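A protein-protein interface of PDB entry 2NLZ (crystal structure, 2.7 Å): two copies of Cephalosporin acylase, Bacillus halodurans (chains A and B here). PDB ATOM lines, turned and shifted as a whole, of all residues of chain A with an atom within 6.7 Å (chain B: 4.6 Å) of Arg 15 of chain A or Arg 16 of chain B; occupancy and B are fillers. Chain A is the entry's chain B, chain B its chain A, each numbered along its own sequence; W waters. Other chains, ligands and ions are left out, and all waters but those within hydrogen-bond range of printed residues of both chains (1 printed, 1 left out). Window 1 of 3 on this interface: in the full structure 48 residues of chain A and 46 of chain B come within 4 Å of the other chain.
NE of Arg 15 of chain B is in hydrogen-bond range of OD1 of Asn 17 of chain B, at 3.1 Å. The side-chain amide oxygen (OE1) of Gln 463 of chain B is in hydrogen-bond range of the backbone NH (N) of Thr 528 of chain B. The side-chain amide oxygen (OD1) of Asn 17 of chain A sits at hydrogen-bond distance from the guanidinium group (NE) of Arg 15 of chain A, at 3.1 Å. The side-chain amide nitrogen (NE2) of Gln 463 of chain A lies within hydrogen-bond range of the side-chain carboxylate (OD1) of Asp 467 of chain A (2.9 Å).
Of the printed residues of chain B, Arg 15 of chain A touches Tyr 10, Arg 16, Glu 506 and Pro 530. Of the printed residues of chain A, Arg 16 of chain B touches Tyr 10 (3.4 Å), Ser 14 (3.6 Å), Arg 15 (2.6 Å), Arg 16 (3.6 Å) and Asn 17 (3.96 Å). Of the printed residues of chain A, Asn 17 of chain B touches Tyr 10 and Thr 532. Of the printed residues of chain B, Asn 17 of chain A touches Tyr 10, Arg 16 and Thr 532. Gly 534 of chain B touches none of the printed residues of chain A. The nearest printed residue of chain B that does not touch Arg 15 of chain A is Ser 14 of chain B (4.1 Å). The nearest printed residue of chain A that does not touch Arg 16 of chain B is Pro 530 of chain A (4.8 Å).
Tyr 10 of chain A touches Arg 16 of chain B, and with the chains exchanged Arg 16 of chain A touches Tyr 10 of chain B. Ser 14 of chain A touches Arg 16 of chain B, and with the chains exchanged Arg 16 of chain A touches Ser 14 of chain B. Ser 14 of chain A touches Pro 530 of chain B, and with the chains exchanged Pro 530 of chain A touches Ser 14 of chain B. Arg 15 of chain A touches Pro 530 of chain B, and with the chains exchanged Pro 530 of chain A touches Arg 15 of chain B.
O of Ser 14 of chain B is in hydrogen-bond range of N of Ser 14 of chain A (2.9 Å). The side-chain hydroxyl (OG) of Ser 14 of chain B is in hydrogen-bond range of the side-chain carboxylate (OD1) of Asp 467 of chain A, at 2.5 Å. The backbone carbonyl oxygen (O) of Arg 15 of chain B sits at hydrogen-bond distance from the guanidinium group (NE) of Arg 16 of chain A. The guanidinium group of Arg 16 of chain B lies within hydrogen-bond range of the backbone carbonyl oxygen of Arg 15 of chain A (2.6 Å). The backbone NH (N) of Val 18 of chain B sits at hydrogen-bond distance from the side-chain hydroxyl (OH) of Tyr 10 of chain A, at 2.8 Å. OE1 of Glu 506 of chain B lies within salt-bridge range of NH1 of Arg 15 of chain A. The backbone carbonyl oxygen (O) of Pro 530 of chain B lies close to the backbone carbonyl oxygen (O) of Arg 15 of chain A (3.5 Å). The backbone carbonyl oxygen (O) of Pro 530 of chain A sits close to the backbone carbonyl oxygen (O) of Arg 15 of chain B (3.4 Å).
Water W1 lies within hydrogen-bond range of O of Thr 532 of chain A (2.7 Å), NH2 of Arg 16 of chain A (2.7 Å), N of Asn 17 of chain B (3.0 Å) and O of Pro 530 of chain A (3.1 Å).
Among the printed residues, merely in contact across the chains: Tyr 10 of chain A with Arg 16 of chain B (3.4 Å), Tyr 10 of chain A with Asn 17 of chain B (3.4 Å), Pro 13 of chain A with Ser 14 of chain B (3.95 Å), Ser 14 of chain A with Arg 16 of chain B (3.6 Å), Ser 14 of chain A with Gln 463 of chain B (3.9 Å), Ser 14 of chain A with Pro 530 of chain B (3.4 Å), Arg 15 of chain A with Tyr 10 of chain B (3.7 Å), Arg 16 of chain A with Tyr 10 of chain B (3.5 Å), Arg 16 of chain A with Ser 14 of chain B (3.9 Å), Arg 16 of chain A with Arg 16 of chain B (3.6 Å), Asn 17 of chain A with Tyr 10 of chain B (3.5 Å), Asn 17 of chain A with Arg 16 of chain B (3.96 Å), Asn 17 of chain A with Thr 532 of chain B (3.5 Å), Gln 463 of chain A with Ser 14 of chain B (3.99 Å), Pro 530 of chain A with Ser 14 of chain B (3.4 Å) and Thr 532 of chain A with Asn 17 of chain B (3.6 Å).
Of the 10 printed residues of chain A, 10 touch a printed residue of chain B. Hydrophobic or aromatic side chains of chain A within 4 Å of the printed part of chain B: Tyr 10 and Pro 530. Along chain A the printed residues that touch a printed residue of chain B span positions 10 to 532. Of the 13 printed residues of chain B, 10 touch a printed residue of chain A. Hydrophobic or aromatic side chains of chain B that line the printed part of chain A: Tyr 10, Val 18 and Pro 530. Among the printed residues, 24 pairs touch across the chains.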
ATOM      1  N   TYR A  10     -19.315 -27.429 -30.170  1.00  0.00           N
ATOM      2  CA  TYR A  10     -19.309 -26.655 -28.929  1.00  0.00           C
ATOM      3  C   TYR A  10     -19.592 -25.169 -29.224  1.00  0.00           C
ATOM      4  O   TYR A  10     -18.667 -24.376 -29.388  1.00  0.00           O
ATOM      5  CB  TYR A  10     -17.977 -26.840 -28.186  1.00  0.00           C
ATOM      6  CG  TYR A  10     -17.618 -28.286 -27.872  1.00  0.00           C
ATOM      7  CD1 TYR A  10     -17.978 -28.865 -26.663  1.00  0.00           C
ATOM      8  CD2 TYR A  10     -16.918 -29.069 -28.782  1.00  0.00           C
ATOM      9  CE1 TYR A  10     -17.653 -30.179 -26.368  1.00  0.00           C
ATOM     10  CE2 TYR A  10     -16.595 -30.382 -28.498  1.00  0.00           C
ATOM     11  CZ  TYR A  10     -16.962 -30.935 -27.287  1.00  0.00           C
ATOM     12  OH  TYR A  10     -16.609 -32.246 -27.008  1.00  0.00           O
ATOM     13  N   PRO A  13     -18.677 -20.943 -25.060  1.00  0.00           N
ATOM     14  CA  PRO A  13     -17.432 -21.042 -24.304  1.00  0.00           C
ATOM     15  C   PRO A  13     -17.619 -21.680 -22.926  1.00  0.00           C
ATOM     16  O   PRO A  13     -18.681 -21.553 -22.313  1.00  0.00           O
ATOM     17  CB  PRO A  13     -16.992 -19.584 -24.172  1.00  0.00           C
ATOM     18  CG  PRO A  13     -18.262 -18.810 -24.221  1.00  0.00           C
ATOM     19  CD  PRO A  13     -19.166 -19.554 -25.145  1.00  0.00           C
ATOM     20  N   SER A  14     -16.581 -22.361 -22.455  1.00  0.00           N
ATOM     21  CA  SER A  14     -16.639 -23.120 -21.209  1.00  0.00           C
ATOM     22  C   SER A  14     -15.616 -22.566 -20.215  1.00  0.00           C
ATOM     23  O   SER A  14     -14.857 -21.660 -20.534  1.00  0.00           O
ATOM     24  CB  SER A  14     -16.403 -24.622 -21.476  1.00  0.00           C
ATOM     25  OG  SER A  14     -16.970 -25.458 -20.472  1.00  0.00           O
ATOM     26  N   ARG A  15     -15.622 -23.115 -19.006  1.00  0.00           N
ATOM     27  CA  ARG A  15     -14.752 -22.671 -17.920  1.00  0.00           C
ATOM     28  C   ARG A  15     -14.073 -23.873 -17.287  1.00  0.00           C
ATOM     29  O   ARG A  15     -14.733 -24.878 -16.998  1.00  0.00           O
ATOM     30  CB  ARG A  15     -15.569 -21.944 -16.841  1.00  0.00           C
ATOM     31  CG  ARG A  15     -15.412 -20.424 -16.759  1.00  0.00           C
ATOM     32  CD  ARG A  15     -14.370 -19.994 -15.715  1.00  0.00           C
ATOM     33  NE  ARG A  15     -14.804 -20.220 -14.336  1.00  0.00           N
ATOM     34  CZ  ARG A  15     -15.050 -19.275 -13.432  1.00  0.00           C
ATOM     35  NH1 ARG A  15     -14.910 -17.988 -13.724  1.00  0.00           N
ATOM     36  NH2 ARG A  15     -15.437 -19.629 -12.217  1.00  0.00           N
ATOM     37  N   ARG A  16     -12.768 -23.767 -17.073  1.00  0.00           N
ATOM     38  CA  ARG A  16     -12.049 -24.747 -16.291  1.00  0.00           C
ATOM     39  C   ARG A  16     -11.480 -24.006 -15.094  1.00  0.00           C
ATOM     40  O   ARG A  16     -10.717 -23.050 -15.255  1.00  0.00           O
ATOM     41  CB  ARG A  16     -10.942 -25.430 -17.101  1.00  0.00           C
ATOM     42  CG  ARG A  16     -11.416 -26.618 -17.908  1.00  0.00           C
ATOM     43  CD  ARG A  16     -10.282 -27.319 -18.601  1.00  0.00           C
ATOM     44  NE  ARG A  16     -10.784 -28.252 -19.601  1.00  0.00           N
ATOM     45  CZ  ARG A  16     -10.912 -29.561 -19.412  1.00  0.00           C
ATOM     46  NH1 ARG A  16     -10.568 -30.109 -18.259  1.00  0.00           N
ATOM     47  NH2 ARG A  16     -11.387 -30.327 -20.383  1.00  0.00           N
ATOM     48  N   ASN A  17     -11.895 -24.416 -13.898  1.00  0.00           N
ATOM     49  CA  ASN A  17     -11.305 -23.914 -12.674  1.00  0.00           C
ATOM     50  C   ASN A  17      -9.989 -24.628 -12.398  1.00  0.00           C
ATOM     51  O   ASN A  17      -9.813 -25.808 -12.735  1.00  0.00           O
ATOM     52  CB  ASN A  17     -12.271 -24.077 -11.489  1.00  0.00           C
ATOM     53  CG  ASN A  17     -13.323 -22.970 -11.420  1.00  0.00           C
ATOM     54  OD1 ASN A  17     -13.335 -22.046 -12.234  1.00  0.00           O
ATOM     55  ND2 ASN A  17     -14.208 -23.061 -10.438  1.00  0.00           N
ATOM     56  N   GLN A 463      -4.279 -22.569 -15.228  1.00  0.00           N
ATOM     57  CA  GLN A 463      -5.317 -22.853 -16.218  1.00  0.00           C
ATOM     58  C   GLN A 463      -5.452 -21.715 -17.212  1.00  0.00           C
ATOM     59  O   GLN A 463      -5.400 -21.935 -18.417  1.00  0.00           O
ATOM     60  CB  GLN A 463      -6.677 -23.120 -15.555  1.00  0.00           C
ATOM     61  CG  GLN A 463      -7.742 -23.619 -16.532  1.00  0.00           C
ATOM     62  CD  GLN A 463      -7.281 -24.854 -17.271  1.00  0.00           C
ATOM     63  OE1 GLN A 463      -6.986 -25.890 -16.669  1.00  0.00           O
ATOM     64  NE2 GLN A 463      -7.219 -24.753 -18.582  1.00  0.00           N
ATOM     65  N   ASP A 467      -5.206 -21.488 -21.111  1.00  0.00           N
ATOM     66  CA  ASP A 467      -6.409 -21.014 -21.808  1.00  0.00           C
ATOM     67  C   ASP A 467      -6.075 -19.949 -22.837  1.00  0.00           C
ATOM     68  O   ASP A 467      -6.689 -19.907 -23.913  1.00  0.00           O
ATOM     69  CB  ASP A 467      -7.440 -20.423 -20.828  1.00  0.00           C
ATOM     70  CG  ASP A 467      -8.091 -21.469 -19.945  1.00  0.00           C
ATOM     71  OD1 ASP A 467      -8.159 -22.657 -20.355  1.00  0.00           O
ATOM     72  OD2 ASP A 467      -8.530 -21.092 -18.830  1.00  0.00           O
ATOM     73  N   PRO A 530      -7.060 -27.139 -22.411  1.00  0.00           N
ATOM     74  CA  PRO A 530      -8.478 -27.134 -22.780  1.00  0.00           C
ATOM     75  C   PRO A 530      -8.758 -27.563 -24.212  1.00  0.00           C
ATOM     76  O   PRO A 530      -9.898 -27.909 -24.522  1.00  0.00           O
ATOM     77  CB  PRO A 530      -8.882 -25.677 -22.595  1.00  0.00           C
ATOM     78  CG  PRO A 530      -7.625 -24.920 -22.835  1.00  0.00           C
ATOM     79  CD  PRO A 530      -6.511 -25.772 -22.320  1.00  0.00           C
ATOM     80  N   THR A 532      -7.940 -30.279 -25.755  1.00  0.00           N
ATOM     81  CA  THR A 532      -7.979 -31.727 -25.941  1.00  0.00           C
ATOM     82  C   THR A 532      -8.639 -32.413 -24.746  1.00  0.00           C
ATOM     83  O   THR A 532      -8.960 -31.743 -23.760  1.00  0.00           O
ATOM     84  CB  THR A 532      -6.550 -32.289 -26.158  1.00  0.00           C
ATOM     85  OG1 THR A 532      -6.619 -33.671 -26.526  1.00  0.00           O
ATOM     86  CG2 THR A 532      -5.699 -32.141 -24.897  1.00  0.00           C
ATOM     87  N   TYR B  10      -9.887 -15.174 -14.603  1.00  0.00           N
ATOM     88  CA  TYR B  10      -9.944 -15.978 -15.818  1.00  0.00           C
ATOM     89  C   TYR B  10     -10.266 -15.087 -17.002  1.00  0.00           C
ATOM     90  O   TYR B  10     -11.426 -14.999 -17.415  1.00  0.00           O
ATOM     91  CB  TYR B  10     -10.996 -17.079 -15.678  1.00  0.00           C
ATOM     92  CG  TYR B  10     -10.684 -18.087 -14.593  1.00  0.00           C
ATOM     93  CD1 TYR B  10      -9.855 -19.176 -14.843  1.00  0.00           C
ATOM     94  CD2 TYR B  10     -11.219 -17.950 -13.316  1.00  0.00           C
ATOM     95  CE1 TYR B  10      -9.569 -20.103 -13.853  1.00  0.00           C
ATOM     96  CE2 TYR B  10     -10.936 -18.871 -12.323  1.00  0.00           C
ATOM     97  CZ  TYR B  10     -10.104 -19.946 -12.598  1.00  0.00           C
ATOM     98  OH  TYR B  10      -9.817 -20.873 -11.621  1.00  0.00           O
ATOM     99  N   SER B  14     -12.412 -20.767 -21.950  1.00  0.00           N
ATOM    100  CA  SER B  14     -11.835 -22.109 -21.965  1.00  0.00           C
ATOM    101  C   SER B  14     -12.746 -23.095 -22.722  1.00  0.00           C
ATOM    102  O   SER B  14     -13.812 -22.713 -23.199  1.00  0.00           O
ATOM    103  CB  SER B  14     -11.547 -22.567 -20.524  1.00  0.00           C
ATOM    104  OG  SER B  14     -10.522 -23.549 -20.471  1.00  0.00           O
ATOM    105  N   ARG B  15     -12.294 -24.343 -22.846  1.00  0.00           N
ATOM    106  CA  ARG B  15     -13.026 -25.408 -23.539  1.00  0.00           C
ATOM    107  C   ARG B  15     -13.083 -26.656 -22.663  1.00  0.00           C
ATOM    108  O   ARG B  15     -12.074 -27.049 -22.069  1.00  0.00           O
ATOM    109  CB  ARG B  15     -12.324 -25.774 -24.857  1.00  0.00           C
ATOM    110  CG  ARG B  15     -12.990 -25.295 -26.152  1.00  0.00           C
ATOM    111  CD  ARG B  15     -13.891 -26.361 -26.800  1.00  0.00           C
ATOM    112  NE  ARG B  15     -13.158 -27.482 -27.389  1.00  0.00           N
ATOM    113  CZ  ARG B  15     -13.028 -27.732 -28.692  1.00  0.00           C
ATOM    114  NH1 ARG B  15     -13.571 -26.944 -29.606  1.00  0.00           N
ATOM    115  NH2 ARG B  15     -12.342 -28.791 -29.083  1.00  0.00           N
ATOM    116  N   ARG B  16     -14.255 -27.277 -22.579  1.00  0.00           N
ATOM    117  CA  ARG B  16     -14.380 -28.599 -21.972  1.00  0.00           C
ATOM    118  C   ARG B  16     -14.917 -29.533 -23.036  1.00  0.00           C
ATOM    119  O   ARG B  16     -16.029 -29.350 -23.521  1.00  0.00           O
ATOM    120  CB  ARG B  16     -15.320 -28.588 -20.765  1.00  0.00           C
ATOM    121  CG  ARG B  16     -14.680 -28.098 -19.494  1.00  0.00           C
ATOM    122  CD  ARG B  16     -15.686 -28.051 -18.340  1.00  0.00           C
ATOM    123  NE  ARG B  16     -15.101 -27.488 -17.114  1.00  0.00           N
ATOM    124  CZ  ARG B  16     -14.435 -28.181 -16.190  1.00  0.00           C
ATOM    125  NH1 ARG B  16     -14.254 -29.488 -16.310  1.00  0.00           N
ATOM    126  NH2 ARG B  16     -13.956 -27.560 -15.133  1.00  0.00           N
ATOM    127  N   ASN B  17     -14.111 -30.509 -23.425  1.00  0.00           N
ATOM    128  CA  ASN B  17     -14.555 -31.537 -24.350  1.00  0.00           C
ATOM    129  C   ASN B  17     -15.421 -32.534 -23.608  1.00  0.00           C
ATOM    130  O   ASN B  17     -15.190 -32.801 -22.419  1.00  0.00           O
ATOM    131  CB  ASN B  17     -13.364 -32.282 -24.982  1.00  0.00           C
ATOM    132  CG  ASN B  17     -12.752 -31.536 -26.165  1.00  0.00           C
ATOM    133  OD1 ASN B  17     -13.260 -30.508 -26.612  1.00  0.00           O
ATOM    134  ND2 ASN B  17     -11.653 -32.063 -26.680  1.00  0.00           N
ATOM    135  N   VAL B  18     -16.415 -33.074 -24.314  1.00  0.00           N
ATOM    136  CA  VAL B  18     -17.254 -34.158 -23.807  1.00  0.00           C
ATOM    137  C   VAL B  18     -16.402 -35.368 -23.389  1.00  0.00           C
ATOM    138  O   VAL B  18     -15.538 -35.835 -24.140  1.00  0.00           O
ATOM    139  CB  VAL B  18     -18.316 -34.590 -24.845  1.00  0.00           C
ATOM    140  CG1 VAL B  18     -19.215 -35.650 -24.287  1.00  0.00           C
ATOM    141  CG2 VAL B  18     -19.150 -33.424 -25.236  1.00  0.00           C
ATOM    142  N   GLN B 463     -21.996 -31.391 -22.543  1.00  0.00           N
ATOM    143  CA  GLN B 463     -21.179 -30.264 -22.101  1.00  0.00           C
ATOM    144  C   GLN B 463     -21.681 -28.922 -22.621  1.00  0.00           C
ATOM    145  O   GLN B 463     -21.910 -28.007 -21.843  1.00  0.00           O
ATOM    146  CB  GLN B 463     -19.740 -30.456 -22.542  1.00  0.00           C
ATOM    147  CG  GLN B 463     -18.807 -29.542 -21.815  1.00  0.00           C
ATOM    148  CD  GLN B 463     -19.035 -29.577 -20.305  1.00  0.00           C
ATOM    149  OE1 GLN B 463     -18.844 -30.615 -19.662  1.00  0.00           O
ATOM    150  NE2 GLN B 463     -19.444 -28.435 -19.734  1.00  0.00           N
ATOM    151  N   GLU B 506     -21.449 -15.243  -9.590  1.00  0.00           N
ATOM    152  CA  GLU B 506     -21.044 -16.584  -9.969  1.00  0.00           C
ATOM    153  C   GLU B 506     -21.874 -17.576  -9.158  1.00  0.00           C
ATOM    154  O   GLU B 506     -22.104 -17.370  -7.964  1.00  0.00           O
ATOM    155  CB  GLU B 506     -19.544 -16.783  -9.713  1.00  0.00           C
ATOM    156  CG  GLU B 506     -18.629 -15.949 -10.626  1.00  0.00           C
ATOM    157  CD  GLU B 506     -17.210 -15.776 -10.083  1.00  0.00           C
ATOM    158  OE1 GLU B 506     -16.251 -15.977 -10.862  1.00  0.00           O
ATOM    159  OE2 GLU B 506     -17.051 -15.433  -8.887  1.00  0.00           O
ATOM    160  N   THR B 528     -19.995 -31.802 -17.544  1.00  0.00           N
ATOM    161  CA  THR B 528     -19.947 -31.293 -16.169  1.00  0.00           C
ATOM    162  C   THR B 528     -20.109 -29.778 -16.096  1.00  0.00           C
ATOM    163  O   THR B 528     -19.822 -29.080 -17.056  1.00  0.00           O
ATOM    164  CB  THR B 528     -18.664 -31.731 -15.431  1.00  0.00           C
ATOM    165  OG1 THR B 528     -18.797 -31.468 -14.026  1.00  0.00           O
ATOM    166  CG2 THR B 528     -17.432 -31.026 -15.996  1.00  0.00           C
ATOM    167  N   PRO B 530     -19.414 -26.124 -15.880  1.00  0.00           N
ATOM    168  CA  PRO B 530     -18.204 -25.307 -15.994  1.00  0.00           C
ATOM    169  C   PRO B 530     -18.129 -24.154 -14.996  1.00  0.00           C
ATOM    170  O   PRO B 530     -17.048 -23.686 -14.703  1.00  0.00           O
ATOM    171  CB  PRO B 530     -18.265 -24.777 -17.428  1.00  0.00           C
ATOM    172  CG  PRO B 530     -19.709 -24.773 -17.759  1.00  0.00           C
ATOM    173  CD  PRO B 530     -20.346 -25.894 -16.994  1.00  0.00           C
ATOM    174  N   ARG B 531     -19.256 -23.716 -14.451  1.00  0.00           N
ATOM    175  CA  ARG B 531     -19.249 -22.592 -13.493  1.00  0.00           C
ATOM    176  C   ARG B 531     -18.712 -22.890 -12.080  1.00  0.00           C
ATOM    177  O   ARG B 531     -18.720 -22.010 -11.225  1.00  0.00           O
ATOM    178  CB  ARG B 531     -20.642 -21.971 -13.388  1.00  0.00           C
ATOM    179  CG  ARG B 531     -21.142 -21.388 -14.685  1.00  0.00           C
ATOM    180  CD  ARG B 531     -22.671 -21.338 -14.708  1.00  0.00           C
ATOM    181  NE  ARG B 531     -23.238 -20.995 -16.019  1.00  0.00           N
ATOM    182  CZ  ARG B 531     -23.394 -21.852 -17.034  1.00  0.00           C
ATOM    183  NH1 ARG B 531     -23.004 -23.117 -16.922  1.00  0.00           N
ATOM    184  NH2 ARG B 531     -23.938 -21.438 -18.176  1.00  0.00           N
ATOM    185  N   THR B 532     -18.241 -24.114 -11.847  1.00  0.00           N
ATOM    186  CA  THR B 532     -17.722 -24.533 -10.535  1.00  0.00           C
ATOM    187  C   THR B 532     -16.610 -25.595 -10.682  1.00  0.00           C
ATOM    188  O   THR B 532     -16.333 -26.049 -11.792  1.00  0.00           O
ATOM    189  CB  THR B 532     -18.872 -25.066  -9.630  1.00  0.00           C
ATOM    190  OG1 THR B 532     -18.400 -25.275  -8.293  1.00  0.00           O
ATOM    191  CG2 THR B 532     -19.427 -26.373 -10.173  1.00  0.00           C
ATOM    192  N   GLY B 534     -15.357 -29.340 -10.444  1.00  0.00           N
ATOM    193  CA  GLY B 534     -16.146 -30.537 -10.680  1.00  0.00           C
ATOM    194  C   GLY B 534     -15.622 -31.355 -11.833  1.00  0.00           C
ATOM    195  O   GLY B 534     -14.688 -30.938 -12.521  1.00  0.00           O
HETATM  196  O   HOH W   1     -11.140 -30.311 -23.104  1.00  0.00           O
